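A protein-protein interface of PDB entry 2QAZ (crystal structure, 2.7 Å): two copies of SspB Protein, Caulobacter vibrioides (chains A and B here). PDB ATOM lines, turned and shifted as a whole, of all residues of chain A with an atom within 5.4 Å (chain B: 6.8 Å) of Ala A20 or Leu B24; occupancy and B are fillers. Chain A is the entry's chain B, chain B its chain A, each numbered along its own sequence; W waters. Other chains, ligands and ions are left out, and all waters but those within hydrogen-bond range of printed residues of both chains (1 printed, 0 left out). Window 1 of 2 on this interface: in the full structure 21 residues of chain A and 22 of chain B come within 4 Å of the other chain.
The backbone NH (N) of Phe B113 is in hydrogen-bond range of the backbone carbonyl oxygen (O) of Leu B122 (2.8 Å).
Val B27 touches Tyr A16.
CE2 of Phe B113 touches CE2 of Tyr A16, 3.6 Å away.
Phe B120 touches Tyr A16 (CD2 to CB, 3.6 Å).
Ala A20 touches Leu B24.
Ala A20 touches Val B27 (CA to CG2, 3.6 Å).
O of Ala A23 touches CB of Ala B23, 3.8 Å away.
Ala B20 touches Leu A24.
Of chain B, only Leu B24 (3.9 Å) and Val B27 (3.6 Å) come within 4 Å of Ala A20.
Of the printed residues of chain B, Ala A23 touches Ala B23.
Of the printed residues of chain B, Leu A24 touches Ala B20 (3.8 Å).
Leu B24 touches just one residue of chain A: Ala A20 (3.9 Å).
Of the printed residues of chain A, Phe B113 touches Tyr A16 (3.6 Å).
Phe B124 touches none of the printed residues of chain A.
The nearest residue of chain B that does not touch Ala A20 is Phe B120 (4.7 Å).
The nearest residue of chain A that does not touch Leu B24 is Leu A24 (4.1 Å).
Of the 10 printed residues of chain A, 4 touch a printed residue of chain B.
Among the printed residues, no Asp or Glu carboxylate lies within 4 Å of a Lys or Arg side-chain nitrogen of the other chain.
Ala A20 touches Leu B24, and with the chains exchanged Leu A24 touches Ala B20.
Ala A23 touches its own counterpart, Ala B23.
6 positions are printed for both chains.
Water W1 bridges O of Ala B23 (3.1 Å) and O of Ala A23 (3.1 Å).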
ATOM      1  N   GLN A  15      12.425 -17.281  21.014  1.00  0.00           N
ATOM      2  CA  GLN A  15      12.291 -18.264  19.947  1.00  0.00           C
ATOM      3  C   GLN A  15      12.432 -17.634  18.559  1.00  0.00           C
ATOM      4  O   GLN A  15      11.649 -17.926  17.651  1.00  0.00           O
ATOM      5  CB  GLN A  15      10.934 -18.966  20.054  1.00  0.00           C
ATOM      6  CG  GLN A  15      10.644 -19.536  21.423  1.00  0.00           C
ATOM      7  CD  GLN A  15       9.549 -20.604  21.408  1.00  0.00           C
ATOM      8  OE1 GLN A  15       8.418 -20.360  20.983  1.00  0.00           O
ATOM      9  NE2 GLN A  15       9.891 -21.798  21.881  1.00  0.00           N
ATOM     10  N   TYR A  16      13.439 -16.782  18.387  1.00  0.00           N
ATOM     11  CA  TYR A  16      13.631 -16.116  17.104  1.00  0.00           C
ATOM     12  C   TYR A  16      13.713 -17.029  15.884  1.00  0.00           C
ATOM     13  O   TYR A  16      13.254 -16.652  14.809  1.00  0.00           O
ATOM     14  CB  TYR A  16      14.853 -15.201  17.153  1.00  0.00           C
ATOM     15  CG  TYR A  16      14.604 -13.956  17.974  1.00  0.00           C
ATOM     16  CD1 TYR A  16      15.242 -13.764  19.203  1.00  0.00           C
ATOM     17  CD2 TYR A  16      13.713 -12.975  17.533  1.00  0.00           C
ATOM     18  CE1 TYR A  16      14.999 -12.632  19.971  1.00  0.00           C
ATOM     19  CE2 TYR A  16      13.458 -11.833  18.298  1.00  0.00           C
ATOM     20  CZ  TYR A  16      14.108 -11.673  19.515  1.00  0.00           C
ATOM     21  OH  TYR A  16      13.870 -10.557  20.278  1.00  0.00           O
ATOM     22  N   GLU A  17      14.280 -18.220  16.032  1.00  0.00           N
ATOM     23  CA  GLU A  17      14.365 -19.121  14.891  1.00  0.00           C
ATOM     24  C   GLU A  17      12.955 -19.496  14.418  1.00  0.00           C
ATOM     25  O   GLU A  17      12.680 -19.532  13.225  1.00  0.00           O
ATOM     26  CB  GLU A  17      15.148 -20.386  15.248  1.00  0.00           C
ATOM     27  CG  GLU A  17      16.526 -20.125  15.832  1.00  0.00           C
ATOM     28  CD  GLU A  17      17.260 -18.966  15.155  1.00  0.00           C
ATOM     29  OE1 GLU A  17      17.346 -18.951  13.902  1.00  0.00           O
ATOM     30  OE2 GLU A  17      17.762 -18.072  15.882  1.00  0.00           O
ATOM     31  N   ALA A  18      12.061 -19.762  15.360  1.00  0.00           N
ATOM     32  CA  ALA A  18      10.700 -20.129  15.012  1.00  0.00           C
ATOM     33  C   ALA A  18       9.980 -18.962  14.358  1.00  0.00           C
ATOM     34  O   ALA A  18       9.349 -19.131  13.320  1.00  0.00           O
ATOM     35  CB  ALA A  18       9.936 -20.592  16.253  1.00  0.00           C
ATOM     36  N   MET A  19      10.062 -17.782  14.965  1.00  0.00           N
ATOM     37  CA  MET A  19       9.407 -16.611  14.403  1.00  0.00           C
ATOM     38  C   MET A  19      10.018 -16.257  13.048  1.00  0.00           C
ATOM     39  O   MET A  19       9.320 -15.773  12.164  1.00  0.00           O
ATOM     40  CB  MET A  19       9.541 -15.403  15.335  1.00  0.00           C
ATOM     41  CG  MET A  19       8.905 -15.546  16.697  1.00  0.00           C
ATOM     42  SD  MET A  19       9.234 -14.071  17.714  1.00  0.00           S
ATOM     43  CE  MET A  19       7.583 -13.525  17.959  1.00  0.00           C
ATOM     44  N   ALA A  20      11.319 -16.485  12.887  1.00  0.00           N
ATOM     45  CA  ALA A  20      11.972 -16.167  11.621  1.00  0.00           C
ATOM     46  C   ALA A  20      11.484 -17.136  10.559  1.00  0.00           C
ATOM     47  O   ALA A  20      11.124 -16.741   9.449  1.00  0.00           O
ATOM     48  CB  ALA A  20      13.488 -16.258  11.755  1.00  0.00           C
ATOM     49  N   GLN A  21      11.475 -18.409  10.924  1.00  0.00           N
ATOM     50  CA  GLN A  21      11.029 -19.475  10.046  1.00  0.00           C
ATOM     51  C   GLN A  21       9.606 -19.164   9.569  1.00  0.00           C
ATOM     52  O   GLN A  21       9.306 -19.232   8.382  1.00  0.00           O
ATOM     53  CB  GLN A  21      11.074 -20.809  10.807  1.00  0.00           C
ATOM     54  CG  GLN A  21      10.903 -22.044   9.939  1.00  0.00           C
ATOM     55  CD  GLN A  21      11.013 -23.351  10.724  1.00  0.00           C
ATOM     56  OE1 GLN A  21      10.194 -23.635  11.605  1.00  0.00           O
ATOM     57  NE2 GLN A  21      12.030 -24.151  10.404  1.00  0.00           N
ATOM     58  N   ASP A  22       8.736 -18.790  10.494  1.00  0.00           N
ATOM     59  CA  ASP A  22       7.358 -18.483  10.144  1.00  0.00           C
ATOM     60  C   ASP A  22       7.243 -17.235   9.266  1.00  0.00           C
ATOM     61  O   ASP A  22       6.405 -17.170   8.365  1.00  0.00           O
ATOM     62  CB  ASP A  22       6.534 -18.284  11.414  1.00  0.00           C
ATOM     63  CG  ASP A  22       5.059 -18.149  11.129  1.00  0.00           C
ATOM     64  OD1 ASP A  22       4.425 -19.163  10.769  1.00  0.00           O
ATOM     65  OD2 ASP A  22       4.524 -17.029  11.248  1.00  0.00           O
ATOM     66  N   ALA A  23       8.083 -16.242   9.531  1.00  0.00           N
ATOM     67  CA  ALA A  23       8.032 -15.008   8.768  1.00  0.00           C
ATOM     68  C   ALA A  23       8.458 -15.228   7.320  1.00  0.00           C
ATOM     69  O   ALA A  23       8.022 -14.508   6.423  1.00  0.00           O
ATOM     70  CB  ALA A  23       8.921 -13.938   9.428  1.00  0.00           C
ATOM     71  N   LEU A  24       9.313 -16.218   7.089  1.00  0.00           N
ATOM     72  CA  LEU A  24       9.770 -16.484   5.737  1.00  0.00           C
ATOM     73  C   LEU A  24       8.655 -17.000   4.818  1.00  0.00           C
ATOM     74  O   LEU A  24       8.818 -17.042   3.594  1.00  0.00           O
ATOM     75  CB  LEU A  24      10.969 -17.435   5.767  1.00  0.00           C
ATOM     76  CG  LEU A  24      12.205 -16.661   6.265  1.00  0.00           C
ATOM     77  CD1 LEU A  24      13.384 -17.595   6.514  1.00  0.00           C
ATOM     78  CD2 LEU A  24      12.567 -15.591   5.231  1.00  0.00           C
ATOM     79  N   MET B  19      14.176 -10.795  -0.981  1.00  0.00           N
ATOM     80  CA  MET B  19      12.802 -11.066  -0.573  1.00  0.00           C
ATOM     81  C   MET B  19      12.808 -11.633   0.845  1.00  0.00           C
ATOM     82  O   MET B  19      11.917 -11.350   1.641  1.00  0.00           O
ATOM     83  CB  MET B  19      12.139 -12.058  -1.529  1.00  0.00           C
ATOM     84  CG  MET B  19      12.117 -11.615  -2.991  1.00  0.00           C
ATOM     85  SD  MET B  19      11.194 -12.769  -4.048  1.00  0.00           S
ATOM     86  CE  MET B  19       9.667 -11.965  -4.130  1.00  0.00           C
ATOM     87  N   ALA B  20      13.821 -12.433   1.159  1.00  0.00           N
ATOM     88  CA  ALA B  20      13.929 -13.022   2.485  1.00  0.00           C
ATOM     89  C   ALA B  20      14.131 -11.918   3.506  1.00  0.00           C
ATOM     90  O   ALA B  20      13.560 -11.939   4.597  1.00  0.00           O
ATOM     91  CB  ALA B  20      15.098 -13.983   2.536  1.00  0.00           C
ATOM     92  N   GLN B  21      14.960 -10.953   3.135  1.00  0.00           N
ATOM     93  CA  GLN B  21      15.274  -9.837   3.998  1.00  0.00           C
ATOM     94  C   GLN B  21      14.033  -8.995   4.289  1.00  0.00           C
ATOM     95  O   GLN B  21      13.761  -8.635   5.435  1.00  0.00           O
ATOM     96  CB  GLN B  21      16.361  -8.996   3.337  1.00  0.00           C
ATOM     97  CG  GLN B  21      16.822  -7.818   4.153  1.00  0.00           C
ATOM     98  CD  GLN B  21      18.073  -7.171   3.579  1.00  0.00           C
ATOM     99  OE1 GLN B  21      19.137  -7.795   3.524  1.00  0.00           O
ATOM    100  NE2 GLN B  21      17.950  -5.917   3.144  1.00  0.00           N
ATOM    101  N   ASP B  22      13.269  -8.686   3.255  1.00  0.00           N
ATOM    102  CA  ASP B  22      12.072  -7.889   3.443  1.00  0.00           C
ATOM    103  C   ASP B  22      11.055  -8.666   4.278  1.00  0.00           C
ATOM    104  O   ASP B  22      10.407  -8.113   5.164  1.00  0.00           O
ATOM    105  CB  ASP B  22      11.485  -7.520   2.079  1.00  0.00           C
ATOM    106  CG  ASP B  22      10.388  -6.497   2.176  1.00  0.00           C
ATOM    107  OD1 ASP B  22      10.625  -5.422   2.768  1.00  0.00           O
ATOM    108  OD2 ASP B  22       9.287  -6.763   1.657  1.00  0.00           O
ATOM    109  N   ALA B  23      10.929  -9.957   4.000  1.00  0.00           N
ATOM    110  CA  ALA B  23       9.991 -10.804   4.725  1.00  0.00           C
ATOM    111  C   ALA B  23      10.338 -10.877   6.210  1.00  0.00           C
ATOM    112  O   ALA B  23       9.443 -10.890   7.064  1.00  0.00           O
ATOM    113  CB  ALA B  23       9.973 -12.212   4.119  1.00  0.00           C
ATOM    114  N   LEU B  24      11.633 -10.935   6.520  1.00  0.00           N
ATOM    115  CA  LEU B  24      12.047 -11.009   7.909  1.00  0.00           C
ATOM    116  C   LEU B  24      11.599  -9.798   8.729  1.00  0.00           C
ATOM    117  O   LEU B  24      11.688  -9.823   9.945  1.00  0.00           O
ATOM    118  CB  LEU B  24      13.559 -11.216   8.015  1.00  0.00           C
ATOM    119  CG  LEU B  24      13.983 -12.661   7.691  1.00  0.00           C
ATOM    120  CD1 LEU B  24      15.479 -12.743   7.619  1.00  0.00           C
ATOM    121  CD2 LEU B  24      13.449 -13.631   8.743  1.00  0.00           C
ATOM    122  N   ARG B  25      11.104  -8.748   8.075  1.00  0.00           N
ATOM    123  CA  ARG B  25      10.592  -7.593   8.820  1.00  0.00           C
ATOM    124  C   ARG B  25       9.497  -8.094   9.753  1.00  0.00           C
ATOM    125  O   ARG B  25       9.202  -7.466  10.765  1.00  0.00           O
ATOM    126  CB  ARG B  25       9.971  -6.540   7.888  1.00  0.00           C
ATOM    127  CG  ARG B  25      10.970  -5.659   7.153  1.00  0.00           C
ATOM    128  CD  ARG B  25      10.287  -4.836   6.077  1.00  0.00           C
ATOM    129  NE  ARG B  25      11.252  -4.284   5.129  1.00  0.00           N
ATOM    130  CZ  ARG B  25      11.954  -3.176   5.331  1.00  0.00           C
ATOM    131  NH1 ARG B  25      11.795  -2.476   6.452  1.00  0.00           N
ATOM    132  NH2 ARG B  25      12.841  -2.787   4.426  1.00  0.00           N
ATOM    133  N   GLY B  26       8.903  -9.232   9.398  1.00  0.00           N
ATOM    134  CA  GLY B  26       7.828  -9.802  10.185  1.00  0.00           C
ATOM    135  C   GLY B  26       8.262 -10.359  11.523  1.00  0.00           C
ATOM    136  O   GLY B  26       7.418 -10.673  12.367  1.00  0.00           O
ATOM    137  N   VAL B  27       9.569 -10.508  11.726  1.00  0.00           N
ATOM    138  CA  VAL B  27      10.042 -11.006  13.003  1.00  0.00           C
ATOM    139  C   VAL B  27       9.825  -9.898  14.024  1.00  0.00           C
ATOM    140  O   VAL B  27       9.404 -10.148  15.157  1.00  0.00           O
ATOM    141  CB  VAL B  27      11.530 -11.364  12.970  1.00  0.00           C
ATOM    142  CG1 VAL B  27      12.001 -11.682  14.394  1.00  0.00           C
ATOM    143  CG2 VAL B  27      11.758 -12.566  12.049  1.00  0.00           C
ATOM    144  N   VAL B  28      10.104  -8.669  13.609  1.00  0.00           N
ATOM    145  CA  VAL B  28       9.920  -7.513  14.479  1.00  0.00           C
ATOM    146  C   VAL B  28       8.464  -7.426  14.918  1.00  0.00           C
ATOM    147  O   VAL B  28       8.169  -7.249  16.104  1.00  0.00           O
ATOM    148  CB  VAL B  28      10.300  -6.211  13.760  1.00  0.00           C
ATOM    149  CG1 VAL B  28      10.120  -5.031  14.692  1.00  0.00           C
ATOM    150  CG2 VAL B  28      11.731  -6.294  13.272  1.00  0.00           C
ATOM    151  N   LYS B  29       7.559  -7.560  13.955  1.00  0.00           N
ATOM    152  CA  LYS B  29       6.121  -7.508  14.218  1.00  0.00           C
ATOM    153  C   LYS B  29       5.724  -8.586  15.236  1.00  0.00           C
ATOM    154  O   LYS B  29       4.983  -8.321  16.183  1.00  0.00           O
ATOM    155  CB  LYS B  29       5.357  -7.732  12.911  1.00  0.00           C
ATOM    156  CG  LYS B  29       3.868  -7.460  12.973  1.00  0.00           C
ATOM    157  CD  LYS B  29       3.064  -8.541  12.242  1.00  0.00           C
ATOM    158  CE  LYS B  29       3.540  -8.801  10.805  1.00  0.00           C
ATOM    159  NZ  LYS B  29       3.289  -7.667   9.857  1.00  0.00           N
ATOM    160  N   PHE B 113      17.257  -4.449  13.482  1.00  0.00           N
ATOM    161  CA  PHE B 113      16.592  -5.074  14.619  1.00  0.00           C
ATOM    162  C   PHE B 113      17.685  -5.823  15.364  1.00  0.00           C
ATOM    163  O   PHE B 113      18.494  -6.510  14.750  1.00  0.00           O
ATOM    164  CB  PHE B 113      15.523  -6.051  14.152  1.00  0.00           C
ATOM    165  CG  PHE B 113      14.858  -6.795  15.269  1.00  0.00           C
ATOM    166  CD1 PHE B 113      13.935  -6.163  16.089  1.00  0.00           C
ATOM    167  CD2 PHE B 113      15.168  -8.132  15.511  1.00  0.00           C
ATOM    168  CE1 PHE B 113      13.322  -6.854  17.146  1.00  0.00           C
ATOM    169  CE2 PHE B 113      14.562  -8.830  16.565  1.00  0.00           C
ATOM    170  CZ  PHE B 113      13.639  -8.188  17.379  1.00  0.00           C
ATOM    171  N   PHE B 120      20.651 -11.649  18.437  1.00  0.00           N
ATOM    172  CA  PHE B 120      19.900 -11.871  17.210  1.00  0.00           C
ATOM    173  C   PHE B 120      19.846 -10.561  16.437  1.00  0.00           C
ATOM    174  O   PHE B 120      19.414  -9.546  16.980  1.00  0.00           O
ATOM    175  CB  PHE B 120      18.486 -12.339  17.536  1.00  0.00           C
ATOM    176  CG  PHE B 120      17.658 -12.607  16.326  1.00  0.00           C
ATOM    177  CD1 PHE B 120      16.728 -11.672  15.882  1.00  0.00           C
ATOM    178  CD2 PHE B 120      17.830 -13.792  15.601  1.00  0.00           C
ATOM    179  CE1 PHE B 120      15.979 -11.907  14.737  1.00  0.00           C
ATOM    180  CE2 PHE B 120      17.091 -14.038  14.460  1.00  0.00           C
ATOM    181  CZ  PHE B 120      16.162 -13.097  14.021  1.00  0.00           C
ATOM    182  N   ALA B 121      20.263 -10.580  15.170  1.00  0.00           N
ATOM    183  CA  ALA B 121      20.291  -9.352  14.369  1.00  0.00           C
ATOM    184  C   ALA B 121      19.649  -9.422  12.985  1.00  0.00           C
ATOM    185  O   ALA B 121      19.746 -10.430  12.295  1.00  0.00           O
ATOM    186  CB  ALA B 121      21.736  -8.878  14.233  1.00  0.00           C
ATOM    187  N   LEU B 122      18.999  -8.339  12.579  1.00  0.00           N
ATOM    188  CA  LEU B 122      18.366  -8.275  11.263  1.00  0.00           C
ATOM    189  C   LEU B 122      18.581  -6.904  10.627  1.00  0.00           C
ATOM    190  O   LEU B 122      18.281  -5.874  11.244  1.00  0.00           O
ATOM    191  CB  LEU B 122      16.857  -8.523  11.357  1.00  0.00           C
ATOM    192  CG  LEU B 122      16.351  -9.909  11.740  1.00  0.00           C
ATOM    193  CD1 LEU B 122      14.833  -9.865  11.935  1.00  0.00           C
ATOM    194  CD2 LEU B 122      16.736 -10.903  10.661  1.00  0.00           C
ATOM    195  N   GLN B 123      19.107  -6.884   9.406  1.00  0.00           N
ATOM    196  CA  GLN B 123      19.298  -5.627   8.699  1.00  0.00           C
ATOM    197  C   GLN B 123      18.221  -5.589   7.610  1.00  0.00           C
ATOM    198  O   GLN B 123      17.887  -6.619   7.029  1.00  0.00           O
ATOM    199  CB  GLN B 123      20.700  -5.550   8.077  1.00  0.00           C
ATOM    200  CG  GLN B 123      21.817  -5.041   9.016  1.00  0.00           C
ATOM    201  CD  GLN B 123      22.254  -6.049  10.100  1.00  0.00           C
ATOM    202  OE1 GLN B 123      22.658  -7.179   9.795  1.00  0.00           O
ATOM    203  NE2 GLN B 123      22.186  -5.632  11.365  1.00  0.00           N
ATOM    204  N   PHE B 124      17.660  -4.412   7.352  1.00  0.00           N
ATOM    205  CA  PHE B 124      16.627  -4.272   6.330  1.00  0.00           C
ATOM    206  C   PHE B 124      17.032  -3.210   5.312  1.00  0.00           C
ATOM    207  O   PHE B 124      17.770  -2.282   5.629  1.00  0.00           O
ATOM    208  CB  PHE B 124      15.301  -3.866   6.968  1.00  0.00           C
ATOM    209  CG  PHE B 124      14.875  -4.752   8.094  1.00  0.00           C
ATOM    210  CD1 PHE B 124      14.817  -4.263   9.399  1.00  0.00           C
ATOM    211  CD2 PHE B 124      14.528  -6.076   7.861  1.00  0.00           C
ATOM    212  CE1 PHE B 124      14.417  -5.085  10.443  1.00  0.00           C
ATOM    213  CE2 PHE B 124      14.127  -6.904   8.910  1.00  0.00           C
ATOM    214  CZ  PHE B 124      14.073  -6.410  10.195  1.00  0.00           C
HETATM  215  O   HOH W   1       6.538 -11.851   6.836  1.00  0.00           O
